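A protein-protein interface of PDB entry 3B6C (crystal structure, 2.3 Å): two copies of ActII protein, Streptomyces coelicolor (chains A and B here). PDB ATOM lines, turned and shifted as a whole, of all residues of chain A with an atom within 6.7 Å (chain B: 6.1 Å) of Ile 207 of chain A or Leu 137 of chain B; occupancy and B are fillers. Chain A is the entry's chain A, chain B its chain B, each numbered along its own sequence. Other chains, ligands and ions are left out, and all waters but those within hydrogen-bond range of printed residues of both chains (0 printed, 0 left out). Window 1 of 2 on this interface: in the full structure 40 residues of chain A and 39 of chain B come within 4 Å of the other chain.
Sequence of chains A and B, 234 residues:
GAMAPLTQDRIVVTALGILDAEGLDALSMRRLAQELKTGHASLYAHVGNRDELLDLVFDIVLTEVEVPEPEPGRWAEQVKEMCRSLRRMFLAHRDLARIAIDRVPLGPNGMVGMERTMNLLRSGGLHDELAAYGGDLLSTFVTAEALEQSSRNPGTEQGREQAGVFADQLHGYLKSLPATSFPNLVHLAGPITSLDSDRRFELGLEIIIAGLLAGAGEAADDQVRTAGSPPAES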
ATOM      1  N   LEU A 137      24.812   6.436   9.949  1.00  0.00           N
ATOM      2  CA  LEU A 137      25.298   6.112   8.620  1.00  0.00           C
ATOM      3  C   LEU A 137      24.221   6.367   7.564  1.00  0.00           C
ATOM      4  O   LEU A 137      24.501   6.945   6.508  1.00  0.00           O
ATOM      5  CB  LEU A 137      25.709   4.636   8.549  1.00  0.00           C
ATOM      6  CG  LEU A 137      26.174   4.121   7.174  1.00  0.00           C
ATOM      7  CD1 LEU A 137      27.333   4.956   6.675  1.00  0.00           C
ATOM      8  CD2 LEU A 137      26.574   2.653   7.276  1.00  0.00           C
ATOM      9  N   PHE A 141      24.427   9.241   4.667  1.00  0.00           N
ATOM     10  CA  PHE A 141      24.413   8.786   3.280  1.00  0.00           C
ATOM     11  C   PHE A 141      23.379   9.578   2.480  1.00  0.00           C
ATOM     12  O   PHE A 141      23.653  10.032   1.380  1.00  0.00           O
ATOM     13  CB  PHE A 141      24.087   7.287   3.264  1.00  0.00           C
ATOM     14  CG  PHE A 141      23.577   6.783   1.949  1.00  0.00           C
ATOM     15  CD1 PHE A 141      24.442   6.591   0.876  1.00  0.00           C
ATOM     16  CD2 PHE A 141      22.212   6.543   1.772  1.00  0.00           C
ATOM     17  CE1 PHE A 141      23.964   6.173  -0.373  1.00  0.00           C
ATOM     18  CE2 PHE A 141      21.721   6.125   0.535  1.00  0.00           C
ATOM     19  CZ  PHE A 141      22.603   5.940  -0.545  1.00  0.00           C
ATOM     20  N   GLU A 145      24.203  12.222  -0.557  1.00  0.00           N
ATOM     21  CA  GLU A 145      23.655  12.062  -1.897  1.00  0.00           C
ATOM     22  C   GLU A 145      22.945  13.343  -2.304  1.00  0.00           C
ATOM     23  O   GLU A 145      23.137  13.839  -3.403  1.00  0.00           O
ATOM     24  CB  GLU A 145      22.671  10.893  -1.969  1.00  0.00           C
ATOM     25  CG  GLU A 145      23.341   9.549  -2.106  1.00  0.00           C
ATOM     26  CD  GLU A 145      24.041   9.379  -3.448  1.00  0.00           C
ATOM     27  OE1 GLU A 145      25.060   8.656  -3.492  1.00  0.00           O
ATOM     28  OE2 GLU A 145      23.564   9.949  -4.456  1.00  0.00           O
ATOM     29  N   ARG A 200      21.838   5.690  -8.168  1.00  0.00           N
ATOM     30  CA  ARG A 200      22.880   5.753  -7.143  1.00  0.00           C
ATOM     31  C   ARG A 200      22.237   5.546  -5.767  1.00  0.00           C
ATOM     32  O   ARG A 200      22.650   4.688  -4.975  1.00  0.00           O
ATOM     33  CB  ARG A 200      23.562   7.140  -7.139  1.00  0.00           C
ATOM     34  CG  ARG A 200      24.612   7.415  -8.208  1.00  0.00           C
ATOM     35  CD  ARG A 200      25.020   8.904  -8.218  1.00  0.00           C
ATOM     36  NE  ARG A 200      25.713   9.358  -7.005  1.00  0.00           N
ATOM     37  CZ  ARG A 200      27.004   9.137  -6.739  1.00  0.00           C
ATOM     38  NH1 ARG A 200      27.770   8.463  -7.601  1.00  0.00           N
ATOM     39  NH2 ARG A 200      27.533   9.582  -5.600  1.00  0.00           N
ATOM     40  N   GLU A 202      19.323   4.257  -4.727  1.00  0.00           N
ATOM     41  CA  GLU A 202      18.829   2.924  -4.384  1.00  0.00           C
ATOM     42  C   GLU A 202      19.951   1.932  -4.150  1.00  0.00           C
ATOM     43  O   GLU A 202      19.915   1.165  -3.182  1.00  0.00           O
ATOM     44  CB  GLU A 202      17.866   2.416  -5.456  1.00  0.00           C
ATOM     45  CG  GLU A 202      16.588   3.261  -5.511  1.00  0.00           C
ATOM     46  CD  GLU A 202      15.753   3.172  -4.231  1.00  0.00           C
ATOM     47  OE1 GLU A 202      15.010   4.132  -3.952  1.00  0.00           O
ATOM     48  OE2 GLU A 202      15.824   2.148  -3.512  1.00  0.00           O
ATOM     49  N   LEU A 203      20.963   1.945  -5.015  1.00  0.00           N
ATOM     50  CA  LEU A 203      22.109   1.039  -4.851  1.00  0.00           C
ATOM     51  C   LEU A 203      22.673   1.251  -3.450  1.00  0.00           C
ATOM     52  O   LEU A 203      22.830   0.306  -2.683  1.00  0.00           O
ATOM     53  CB  LEU A 203      23.191   1.359  -5.875  1.00  0.00           C
ATOM     54  CG  LEU A 203      22.968   0.842  -7.284  1.00  0.00           C
ATOM     55  CD1 LEU A 203      24.070   1.378  -8.220  1.00  0.00           C
ATOM     56  CD2 LEU A 203      22.995  -0.675  -7.246  1.00  0.00           C
ATOM     57  N   GLY A 204      22.953   2.513  -3.132  1.00  0.00           N
ATOM     58  CA  GLY A 204      23.496   2.865  -1.838  1.00  0.00           C
ATOM     59  C   GLY A 204      22.613   2.408  -0.703  1.00  0.00           C
ATOM     60  O   GLY A 204      23.108   1.990   0.342  1.00  0.00           O
ATOM     61  N   LEU A 205      21.299   2.479  -0.900  1.00  0.00           N
ATOM     62  CA  LEU A 205      20.362   2.061   0.136  1.00  0.00           C
ATOM     63  C   LEU A 205      20.415   0.582   0.357  1.00  0.00           C
ATOM     64  O   LEU A 205      20.497   0.119   1.500  1.00  0.00           O
ATOM     65  CB  LEU A 205      18.925   2.419  -0.223  1.00  0.00           C
ATOM     66  CG  LEU A 205      18.353   3.713   0.343  1.00  0.00           C
ATOM     67  CD1 LEU A 205      16.855   3.724   0.058  1.00  0.00           C
ATOM     68  CD2 LEU A 205      18.629   3.813   1.856  1.00  0.00           C
ATOM     69  N   GLU A 206      20.345  -0.171  -0.729  1.00  0.00           N
ATOM     70  CA  GLU A 206      20.365  -1.613  -0.592  1.00  0.00           C
ATOM     71  C   GLU A 206      21.673  -2.128  -0.016  1.00  0.00           C
ATOM     72  O   GLU A 206      21.674  -3.113   0.711  1.00  0.00           O
ATOM     73  CB  GLU A 206      20.076  -2.304  -1.922  1.00  0.00           C
ATOM     74  CG  GLU A 206      19.910  -3.817  -1.760  1.00  0.00           C
ATOM     75  CD  GLU A 206      18.850  -4.201  -0.718  1.00  0.00           C
ATOM     76  OE1 GLU A 206      17.656  -3.880  -0.919  1.00  0.00           O
ATOM     77  OE2 GLU A 206      19.216  -4.822   0.304  1.00  0.00           O
ATOM     78  N   ILE A 207      22.788  -1.475  -0.334  1.00  0.00           N
ATOM     79  CA  ILE A 207      24.065  -1.912   0.214  1.00  0.00           C
ATOM     80  C   ILE A 207      24.024  -1.746   1.730  1.00  0.00           C
ATOM     81  O   ILE A 207      24.220  -2.700   2.475  1.00  0.00           O
ATOM     82  CB  ILE A 207      25.233  -1.082  -0.327  1.00  0.00           C
ATOM     83  CG1 ILE A 207      25.419  -1.339  -1.823  1.00  0.00           C
ATOM     84  CG2 ILE A 207      26.497  -1.423   0.435  1.00  0.00           C
ATOM     85  CD1 ILE A 207      26.412  -0.392  -2.487  1.00  0.00           C
ATOM     86  N   ILE A 208      23.754  -0.531   2.185  1.00  0.00           N
ATOM     87  CA  ILE A 208      23.716  -0.256   3.612  1.00  0.00           C
ATOM     88  C   ILE A 208      22.681  -1.072   4.404  1.00  0.00           C
ATOM     89  O   ILE A 208      22.974  -1.540   5.503  1.00  0.00           O
ATOM     90  CB  ILE A 208      23.503   1.248   3.863  1.00  0.00           C
ATOM     91  CG1 ILE A 208      24.646   2.035   3.215  1.00  0.00           C
ATOM     92  CG2 ILE A 208      23.448   1.519   5.359  1.00  0.00           C
ATOM     93  CD1 ILE A 208      24.513   3.533   3.310  1.00  0.00           C
ATOM     94  N   ILE A 209      21.481  -1.244   3.858  1.00  0.00           N
ATOM     95  CA  ILE A 209      20.460  -2.024   4.552  1.00  0.00           C
ATOM     96  C   ILE A 209      20.860  -3.513   4.608  1.00  0.00           C
ATOM     97  O   ILE A 209      20.649  -4.174   5.620  1.00  0.00           O
ATOM     98  CB  ILE A 209      19.081  -1.856   3.874  1.00  0.00           C
ATOM     99  CG1 ILE A 209      18.513  -0.485   4.227  1.00  0.00           C
ATOM    100  CG2 ILE A 209      18.125  -2.933   4.332  1.00  0.00           C
ATOM    101  CD1 ILE A 209      17.219  -0.165   3.532  1.00  0.00           C
ATOM    102  N   ALA A 210      21.453  -4.031   3.533  1.00  0.00           N
ATOM    103  CA  ALA A 210      21.878  -5.427   3.504  1.00  0.00           C
ATOM    104  C   ALA A 210      22.957  -5.650   4.571  1.00  0.00           C
ATOM    105  O   ALA A 210      22.962  -6.684   5.267  1.00  0.00           O
ATOM    106  CB  ALA A 210      22.420  -5.796   2.118  1.00  0.00           C
ATOM    107  N   GLY A 211      23.859  -4.672   4.696  1.00  0.00           N
ATOM    108  CA  GLY A 211      24.937  -4.764   5.668  1.00  0.00           C
ATOM    109  C   GLY A 211      24.441  -4.677   7.093  1.00  0.00           C
ATOM    110  O   GLY A 211      24.972  -5.318   7.986  1.00  0.00           O
ATOM    111  N   LEU A 212      23.419  -3.864   7.322  1.00  0.00           N
ATOM    112  CA  LEU A 212      22.868  -3.730   8.664  1.00  0.00           C
ATOM    113  C   LEU A 212      22.251  -5.068   9.043  1.00  0.00           C
ATOM    114  O   LEU A 212      22.396  -5.529  10.169  1.00  0.00           O
ATOM    115  CB  LEU A 212      21.835  -2.604   8.704  1.00  0.00           C
ATOM    116  CG  LEU A 212      22.431  -1.193   8.623  1.00  0.00           C
ATOM    117  CD1 LEU A 212      21.321  -0.153   8.590  1.00  0.00           C
ATOM    118  CD2 LEU A 212      23.336  -0.949   9.815  1.00  0.00           C
ATOM    119  N   LEU B 130      27.605  -1.819  -9.461  1.00  0.00           N
ATOM    120  CA  LEU B 130      27.938  -2.104  -8.071  1.00  0.00           C
ATOM    121  C   LEU B 130      29.390  -1.748  -7.768  1.00  0.00           C
ATOM    122  O   LEU B 130      29.695  -1.187  -6.716  1.00  0.00           O
ATOM    123  CB  LEU B 130      27.680  -3.576  -7.750  1.00  0.00           C
ATOM    124  CG  LEU B 130      26.986  -3.869  -6.417  1.00  0.00           C
ATOM    125  CD1 LEU B 130      27.434  -5.211  -5.860  1.00  0.00           C
ATOM    126  CD2 LEU B 130      27.250  -2.753  -5.417  1.00  0.00           C
ATOM    127  N   ALA B 132      31.382   0.354  -9.730  1.00  0.00           N
ATOM    128  CA  ALA B 132      31.499   1.787  -9.936  1.00  0.00           C
ATOM    129  C   ALA B 132      30.988   2.559  -8.721  1.00  0.00           C
ATOM    130  O   ALA B 132      31.687   3.427  -8.197  1.00  0.00           O
ATOM    131  CB  ALA B 132      30.712   2.202 -11.173  1.00  0.00           C
ATOM    132  N   TYR B 133      29.784   2.224  -8.263  1.00  0.00           N
ATOM    133  CA  TYR B 133      29.186   2.913  -7.127  1.00  0.00           C
ATOM    134  C   TYR B 133      29.829   2.580  -5.778  1.00  0.00           C
ATOM    135  O   TYR B 133      30.052   3.470  -4.946  1.00  0.00           O
ATOM    136  CB  TYR B 133      27.675   2.634  -7.064  1.00  0.00           C
ATOM    137  CG  TYR B 133      26.999   3.489  -6.028  1.00  0.00           C
ATOM    138  CD1 TYR B 133      26.988   4.878  -6.156  1.00  0.00           C
ATOM    139  CD2 TYR B 133      26.472   2.930  -4.861  1.00  0.00           C
ATOM    140  CE1 TYR B 133      26.478   5.693  -5.146  1.00  0.00           C
ATOM    141  CE2 TYR B 133      25.966   3.737  -3.841  1.00  0.00           C
ATOM    142  CZ  TYR B 133      25.974   5.114  -3.989  1.00  0.00           C
ATOM    143  OH  TYR B 133      25.510   5.929  -2.981  1.00  0.00           O
ATOM    144  N   GLY B 134      30.118   1.296  -5.567  1.00  0.00           N
ATOM    145  CA  GLY B 134      30.742   0.856  -4.322  1.00  0.00           C
ATOM    146  C   GLY B 134      31.990   1.665  -4.019  1.00  0.00           C
ATOM    147  O   GLY B 134      32.216   2.073  -2.890  1.00  0.00           O
ATOM    148  N   GLY B 135      32.811   1.881  -5.044  1.00  0.00           N
ATOM    149  CA  GLY B 135      34.023   2.679  -4.912  1.00  0.00           C
ATOM    150  C   GLY B 135      33.653   4.097  -4.496  1.00  0.00           C
ATOM    151  O   GLY B 135      34.351   4.726  -3.700  1.00  0.00           O
ATOM    152  N   ASP B 136      32.585   4.619  -5.083  1.00  0.00           N
ATOM    153  CA  ASP B 136      32.100   5.937  -4.733  1.00  0.00           C
ATOM    154  C   ASP B 136      31.644   5.903  -3.251  1.00  0.00           C
ATOM    155  O   ASP B 136      32.039   6.750  -2.450  1.00  0.00           O
ATOM    156  CB  ASP B 136      30.886   6.304  -5.587  1.00  0.00           C
ATOM    157  CG  ASP B 136      30.718   7.805  -5.745  1.00  0.00           C
ATOM    158  OD1 ASP B 136      30.874   8.534  -4.739  1.00  0.00           O
ATOM    159  OD2 ASP B 136      30.433   8.253  -6.878  1.00  0.00           O
ATOM    160  N   LEU B 137      30.834   4.908  -2.892  1.00  0.00           N
ATOM    161  CA  LEU B 137      30.323   4.795  -1.535  1.00  0.00           C
ATOM    162  C   LEU B 137      31.426   4.730  -0.492  1.00  0.00           C
ATOM    163  O   LEU B 137      31.393   5.472   0.498  1.00  0.00           O
ATOM    164  CB  LEU B 137      29.433   3.550  -1.398  1.00  0.00           C
ATOM    165  CG  LEU B 137      28.117   3.729  -0.612  1.00  0.00           C
ATOM    166  CD1 LEU B 137      27.698   2.402   0.020  1.00  0.00           C
ATOM    167  CD2 LEU B 137      28.278   4.811   0.456  1.00  0.00           C
ATOM    168  N   LEU B 138      32.408   3.855  -0.721  1.00  0.00           N
ATOM    169  CA  LEU B 138      33.509   3.684   0.225  1.00  0.00           C
ATOM    170  C   LEU B 138      34.290   4.962   0.395  1.00  0.00           C
ATOM    171  O   LEU B 138      34.613   5.364   1.515  1.00  0.00           O
ATOM    172  CB  LEU B 138      34.419   2.529  -0.217  1.00  0.00           C
ATOM    173  CG  LEU B 138      33.813   1.119  -0.142  1.00  0.00           C
ATOM    174  CD1 LEU B 138      34.702   0.142  -0.889  1.00  0.00           C
ATOM    175  CD2 LEU B 138      33.639   0.702   1.311  1.00  0.00           C
ATOM    176  N   SER B 139      34.602   5.601  -0.716  1.00  0.00           N
ATOM    177  CA  SER B 139      35.343   6.856  -0.682  1.00  0.00           C
ATOM    178  C   SER B 139      34.556   7.899   0.128  1.00  0.00           C
ATOM    179  O   SER B 139      35.114   8.587   0.976  1.00  0.00           O
ATOM    180  CB  SER B 139      35.551   7.379  -2.117  1.00  0.00           C
ATOM    181  OG  SER B 139      36.845   7.943  -2.259  1.00  0.00           O
ATOM    182  N   THR B 140      33.260   8.006  -0.143  1.00  0.00           N
ATOM    183  CA  THR B 140      32.405   8.960   0.544  1.00  0.00           C
ATOM    184  C   THR B 140      32.377   8.654   2.023  1.00  0.00           C
ATOM    185  O   THR B 140      32.483   9.543   2.863  1.00  0.00           O
ATOM    186  CB  THR B 140      30.987   8.901  -0.045  1.00  0.00           C
ATOM    187  OG1 THR B 140      31.037   9.321  -1.412  1.00  0.00           O
ATOM    188  CG2 THR B 140      30.038   9.805   0.724  1.00  0.00           C
ATOM    189  N   PHE B 141      32.235   7.381   2.340  1.00  0.00           N
ATOM    190  CA  PHE B 141      32.211   6.953   3.720  1.00  0.00           C
ATOM    191  C   PHE B 141      33.479   7.342   4.466  1.00  0.00           C
ATOM    192  O   PHE B 141      33.429   7.937   5.537  1.00  0.00           O
ATOM    193  CB  PHE B 141      32.067   5.445   3.795  1.00  0.00           C
ATOM    194  CG  PHE B 141      32.297   4.902   5.160  1.00  0.00           C
ATOM    195  CD1 PHE B 141      31.383   5.150   6.173  1.00  0.00           C
ATOM    196  CD2 PHE B 141      33.450   4.184   5.455  1.00  0.00           C
ATOM    197  CE1 PHE B 141      31.612   4.696   7.477  1.00  0.00           C
ATOM    198  CE2 PHE B 141      33.696   3.727   6.755  1.00  0.00           C
ATOM    199  CZ  PHE B 141      32.775   3.984   7.765  1.00  0.00           C
ATOM    200  N   VAL B 142      34.626   6.992   3.909  1.00  0.00           N
ATOM    201  CA  VAL B 142      35.874   7.278   4.582  1.00  0.00           C
ATOM    202  C   VAL B 142      36.099   8.754   4.765  1.00  0.00           C
ATOM    203  O   VAL B 142      36.556   9.196   5.822  1.00  0.00           O
ATOM    204  CB  VAL B 142      37.071   6.686   3.822  1.00  0.00           C
ATOM    205  CG1 VAL B 142      38.358   7.222   4.395  1.00  0.00           C
ATOM    206  CG2 VAL B 142      37.057   5.169   3.942  1.00  0.00           C
ATOM    207  N   ILE B 207      29.696  -2.715   7.574  1.00  0.00           N
ATOM    208  CA  ILE B 207      28.353  -2.567   7.034  1.00  0.00           C
ATOM    209  C   ILE B 207      28.358  -2.434   5.527  1.00  0.00           C
ATOM    210  O   ILE B 207      27.653  -3.157   4.834  1.00  0.00           O
ATOM    211  CB  ILE B 207      27.619  -1.354   7.661  1.00  0.00           C
ATOM    212  CG1 ILE B 207      27.294  -1.658   9.127  1.00  0.00           C
ATOM    213  CG2 ILE B 207      26.325  -1.059   6.889  1.00  0.00           C
ATOM    214  CD1 ILE B 207      26.620  -0.537   9.849  1.00  0.00           C
ATOM    215  N   ILE B 208      29.154  -1.512   5.011  1.00  0.00           N
ATOM    216  CA  ILE B 208      29.211  -1.329   3.573  1.00  0.00           C
ATOM    217  C   ILE B 208      29.761  -2.569   2.871  1.00  0.00           C
ATOM    218  O   ILE B 208      29.193  -3.048   1.891  1.00  0.00           O
ATOM    219  CB  ILE B 208      30.058  -0.093   3.228  1.00  0.00           C
ATOM    220  CG1 ILE B 208      29.340   1.152   3.749  1.00  0.00           C
ATOM    221  CG2 ILE B 208      30.282  -0.001   1.717  1.00  0.00           C
ATOM    222  CD1 ILE B 208      30.162   2.417   3.690  1.00  0.00           C
ATOM    223  N   ILE B 209      30.855  -3.115   3.377  1.00  0.00           N
ATOM    224  CA  ILE B 209      31.438  -4.300   2.744  1.00  0.00           C
ATOM    225  C   ILE B 209      30.477  -5.491   2.658  1.00  0.00           C
ATOM    226  O   ILE B 209      30.411  -6.187   1.636  1.00  0.00           O
ATOM    227  CB  ILE B 209      32.697  -4.758   3.488  1.00  0.00           C
ATOM    228  CG1 ILE B 209      33.829  -3.754   3.278  1.00  0.00           C
ATOM    229  CG2 ILE B 209      33.131  -6.132   2.983  1.00  0.00           C
ATOM    230  CD1 ILE B 209      34.306  -3.739   1.899  1.00  0.00           C
ATOM    231  N   ALA B 210      29.744  -5.739   3.740  1.00  0.00           N
ATOM    232  CA  ALA B 210      28.803  -6.850   3.774  1.00  0.00           C
ATOM    233  C   ALA B 210      27.688  -6.590   2.775  1.00  0.00           C
ATOM    234  O   ALA B 210      27.174  -7.516   2.141  1.00  0.00           O
ATOM    235  CB  ALA B 210      28.232  -7.012   5.183  1.00  0.00           C
ATOM    236  N   GLY B 211      27.331  -5.319   2.626  1.00  0.00           N
ATOM    237  CA  GLY B 211      26.288  -4.951   1.696  1.00  0.00           C
ATOM    238  C   GLY B 211      26.716  -5.201   0.274  1.00  0.00           C
ATOM    239  O   GLY B 211      25.927  -5.689  -0.529  1.00  0.00           O
ATOM    240  N   LEU B 212      27.960  -4.849  -0.048  1.00  0.00           N
ATOM    241  CA  LEU B 212      28.498  -5.056  -1.397  1.00  0.00           C
ATOM    242  C   LEU B 212      28.516  -6.553  -1.727  1.00  0.00           C
ATOM    243  O   LEU B 212      28.101  -6.962  -2.819  1.00  0.00           O
ATOM    244  CB  LEU B 212      29.904  -4.485  -1.493  1.00  0.00           C
ATOM    245  CG  LEU B 212      30.015  -2.962  -1.328  1.00  0.00           C
ATOM    246  CD1 LEU B 212      31.477  -2.558  -1.135  1.00  0.00           C
ATOM    247  CD2 LEU B 212      29.428  -2.271  -2.554  1.00  0.00           C
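Ile 207 of chain B touches Leu 137 of chain A (CG2 to CD2, 3.7 Å).
Arg 200 of chain A touches Tyr 133 of chain B.
CB of Leu 203 of chain A touches CD2 of Tyr 133 of chain B, at 3.8 Å.
Tyr 133 of chain B touches Gly 204 of chain A.
Ile 207 of chain A touches Leu 130 of chain B (CD1 to CD2, 3.9 Å).
Ile 207 of chain A touches Leu 137 of chain B.
Ile 207 of chain A touches Gly 211 of chain B.
CD1 of Ile 207 of chain A touches CD2 of Leu 212 of chain B (3.6 Å).
CB of Ala 210 of chain A touches CA of Gly 211 of chain B, at 3.98 Å.
Ile 207 of chain B touches Leu 212 of chain A (CD1 to CD2, 3.3 Å).
The side-chain carboxylate of Glu 145 of chain A is in salt-bridge range of the guanidinium group of Arg 200 of chain A (3.4 Å).
The backbone carbonyl oxygen of Asp 136 of chain B sits at hydrogen-bond distance from the side-chain hydroxyl of Thr 140 of chain B (2.9 Å).
OH of Tyr 133 of chain B sits at hydrogen-bond distance from OE1 of Glu 145 of chain A (2.8 Å).
OD2 of Asp 136 of chain B is in salt-bridge range of NH1 of Arg 200 of chain A (2.8 Å).
Hydrophobic or aromatic side chains of chain A that line the printed part of chain B: Leu 137, Phe 141, Leu 203, Ile 207, Ala 210 and Leu 212.
Among the printed residues, 17 pairs touch across the chains.
Among the printed residues, Asp or Glu carboxylates within 4 Å of a Lys or Arg side-chain nitrogen of the other chain: Arg 200 of chain A with Asp 136 of chain B (2.8 Å).
Printed residues of chain B within 4 Å of Ile 207 of chain A: Leu 130, Leu 137, Ile 208, Gly 211 and Leu 212.
Printed residues of chain B within 4 Å of Leu 212 of chain A: Ile 207 (3.3 Å).
Of the printed residues of chain A, Asp 136 of chain B touches Arg 200.
Of chain A, only Ile 207 (3.97 Å) comes within 4 Å of Leu 137 of chain B.
Of the printed residues of chain A, Ile 207 of chain B touches Leu 137, Ile 208, Gly 211 and Leu 212.
Of the printed residues of chain A, Leu 212 of chain B touches Ile 207.
The nearest residue of chain B that does not touch Ile 207 of chain A is Tyr 133 of chain B (4.1 Å).
Ile 207 of chain A touches Gly 211 of chain B, and with the chains exchanged Gly 211 of chain A touches Ile 207 of chain B.
Ile 207 of chain A touches Leu 212 of chain B, and with the chains exchanged Leu 212 of chain A touches Ile 207 of chain B.
Ala 210 of chain A touches Gly 211 of chain B, but with the chains exchanged Gly 211 of chain A does not touch Ala 210 of chain B (4.02 Å).
Gly 211 of chain B touches its own counterpart, Gly 211 of chain A.
Positions printed for both chains: 137, 141, 207, 208, 209, 210, 211 and 212.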
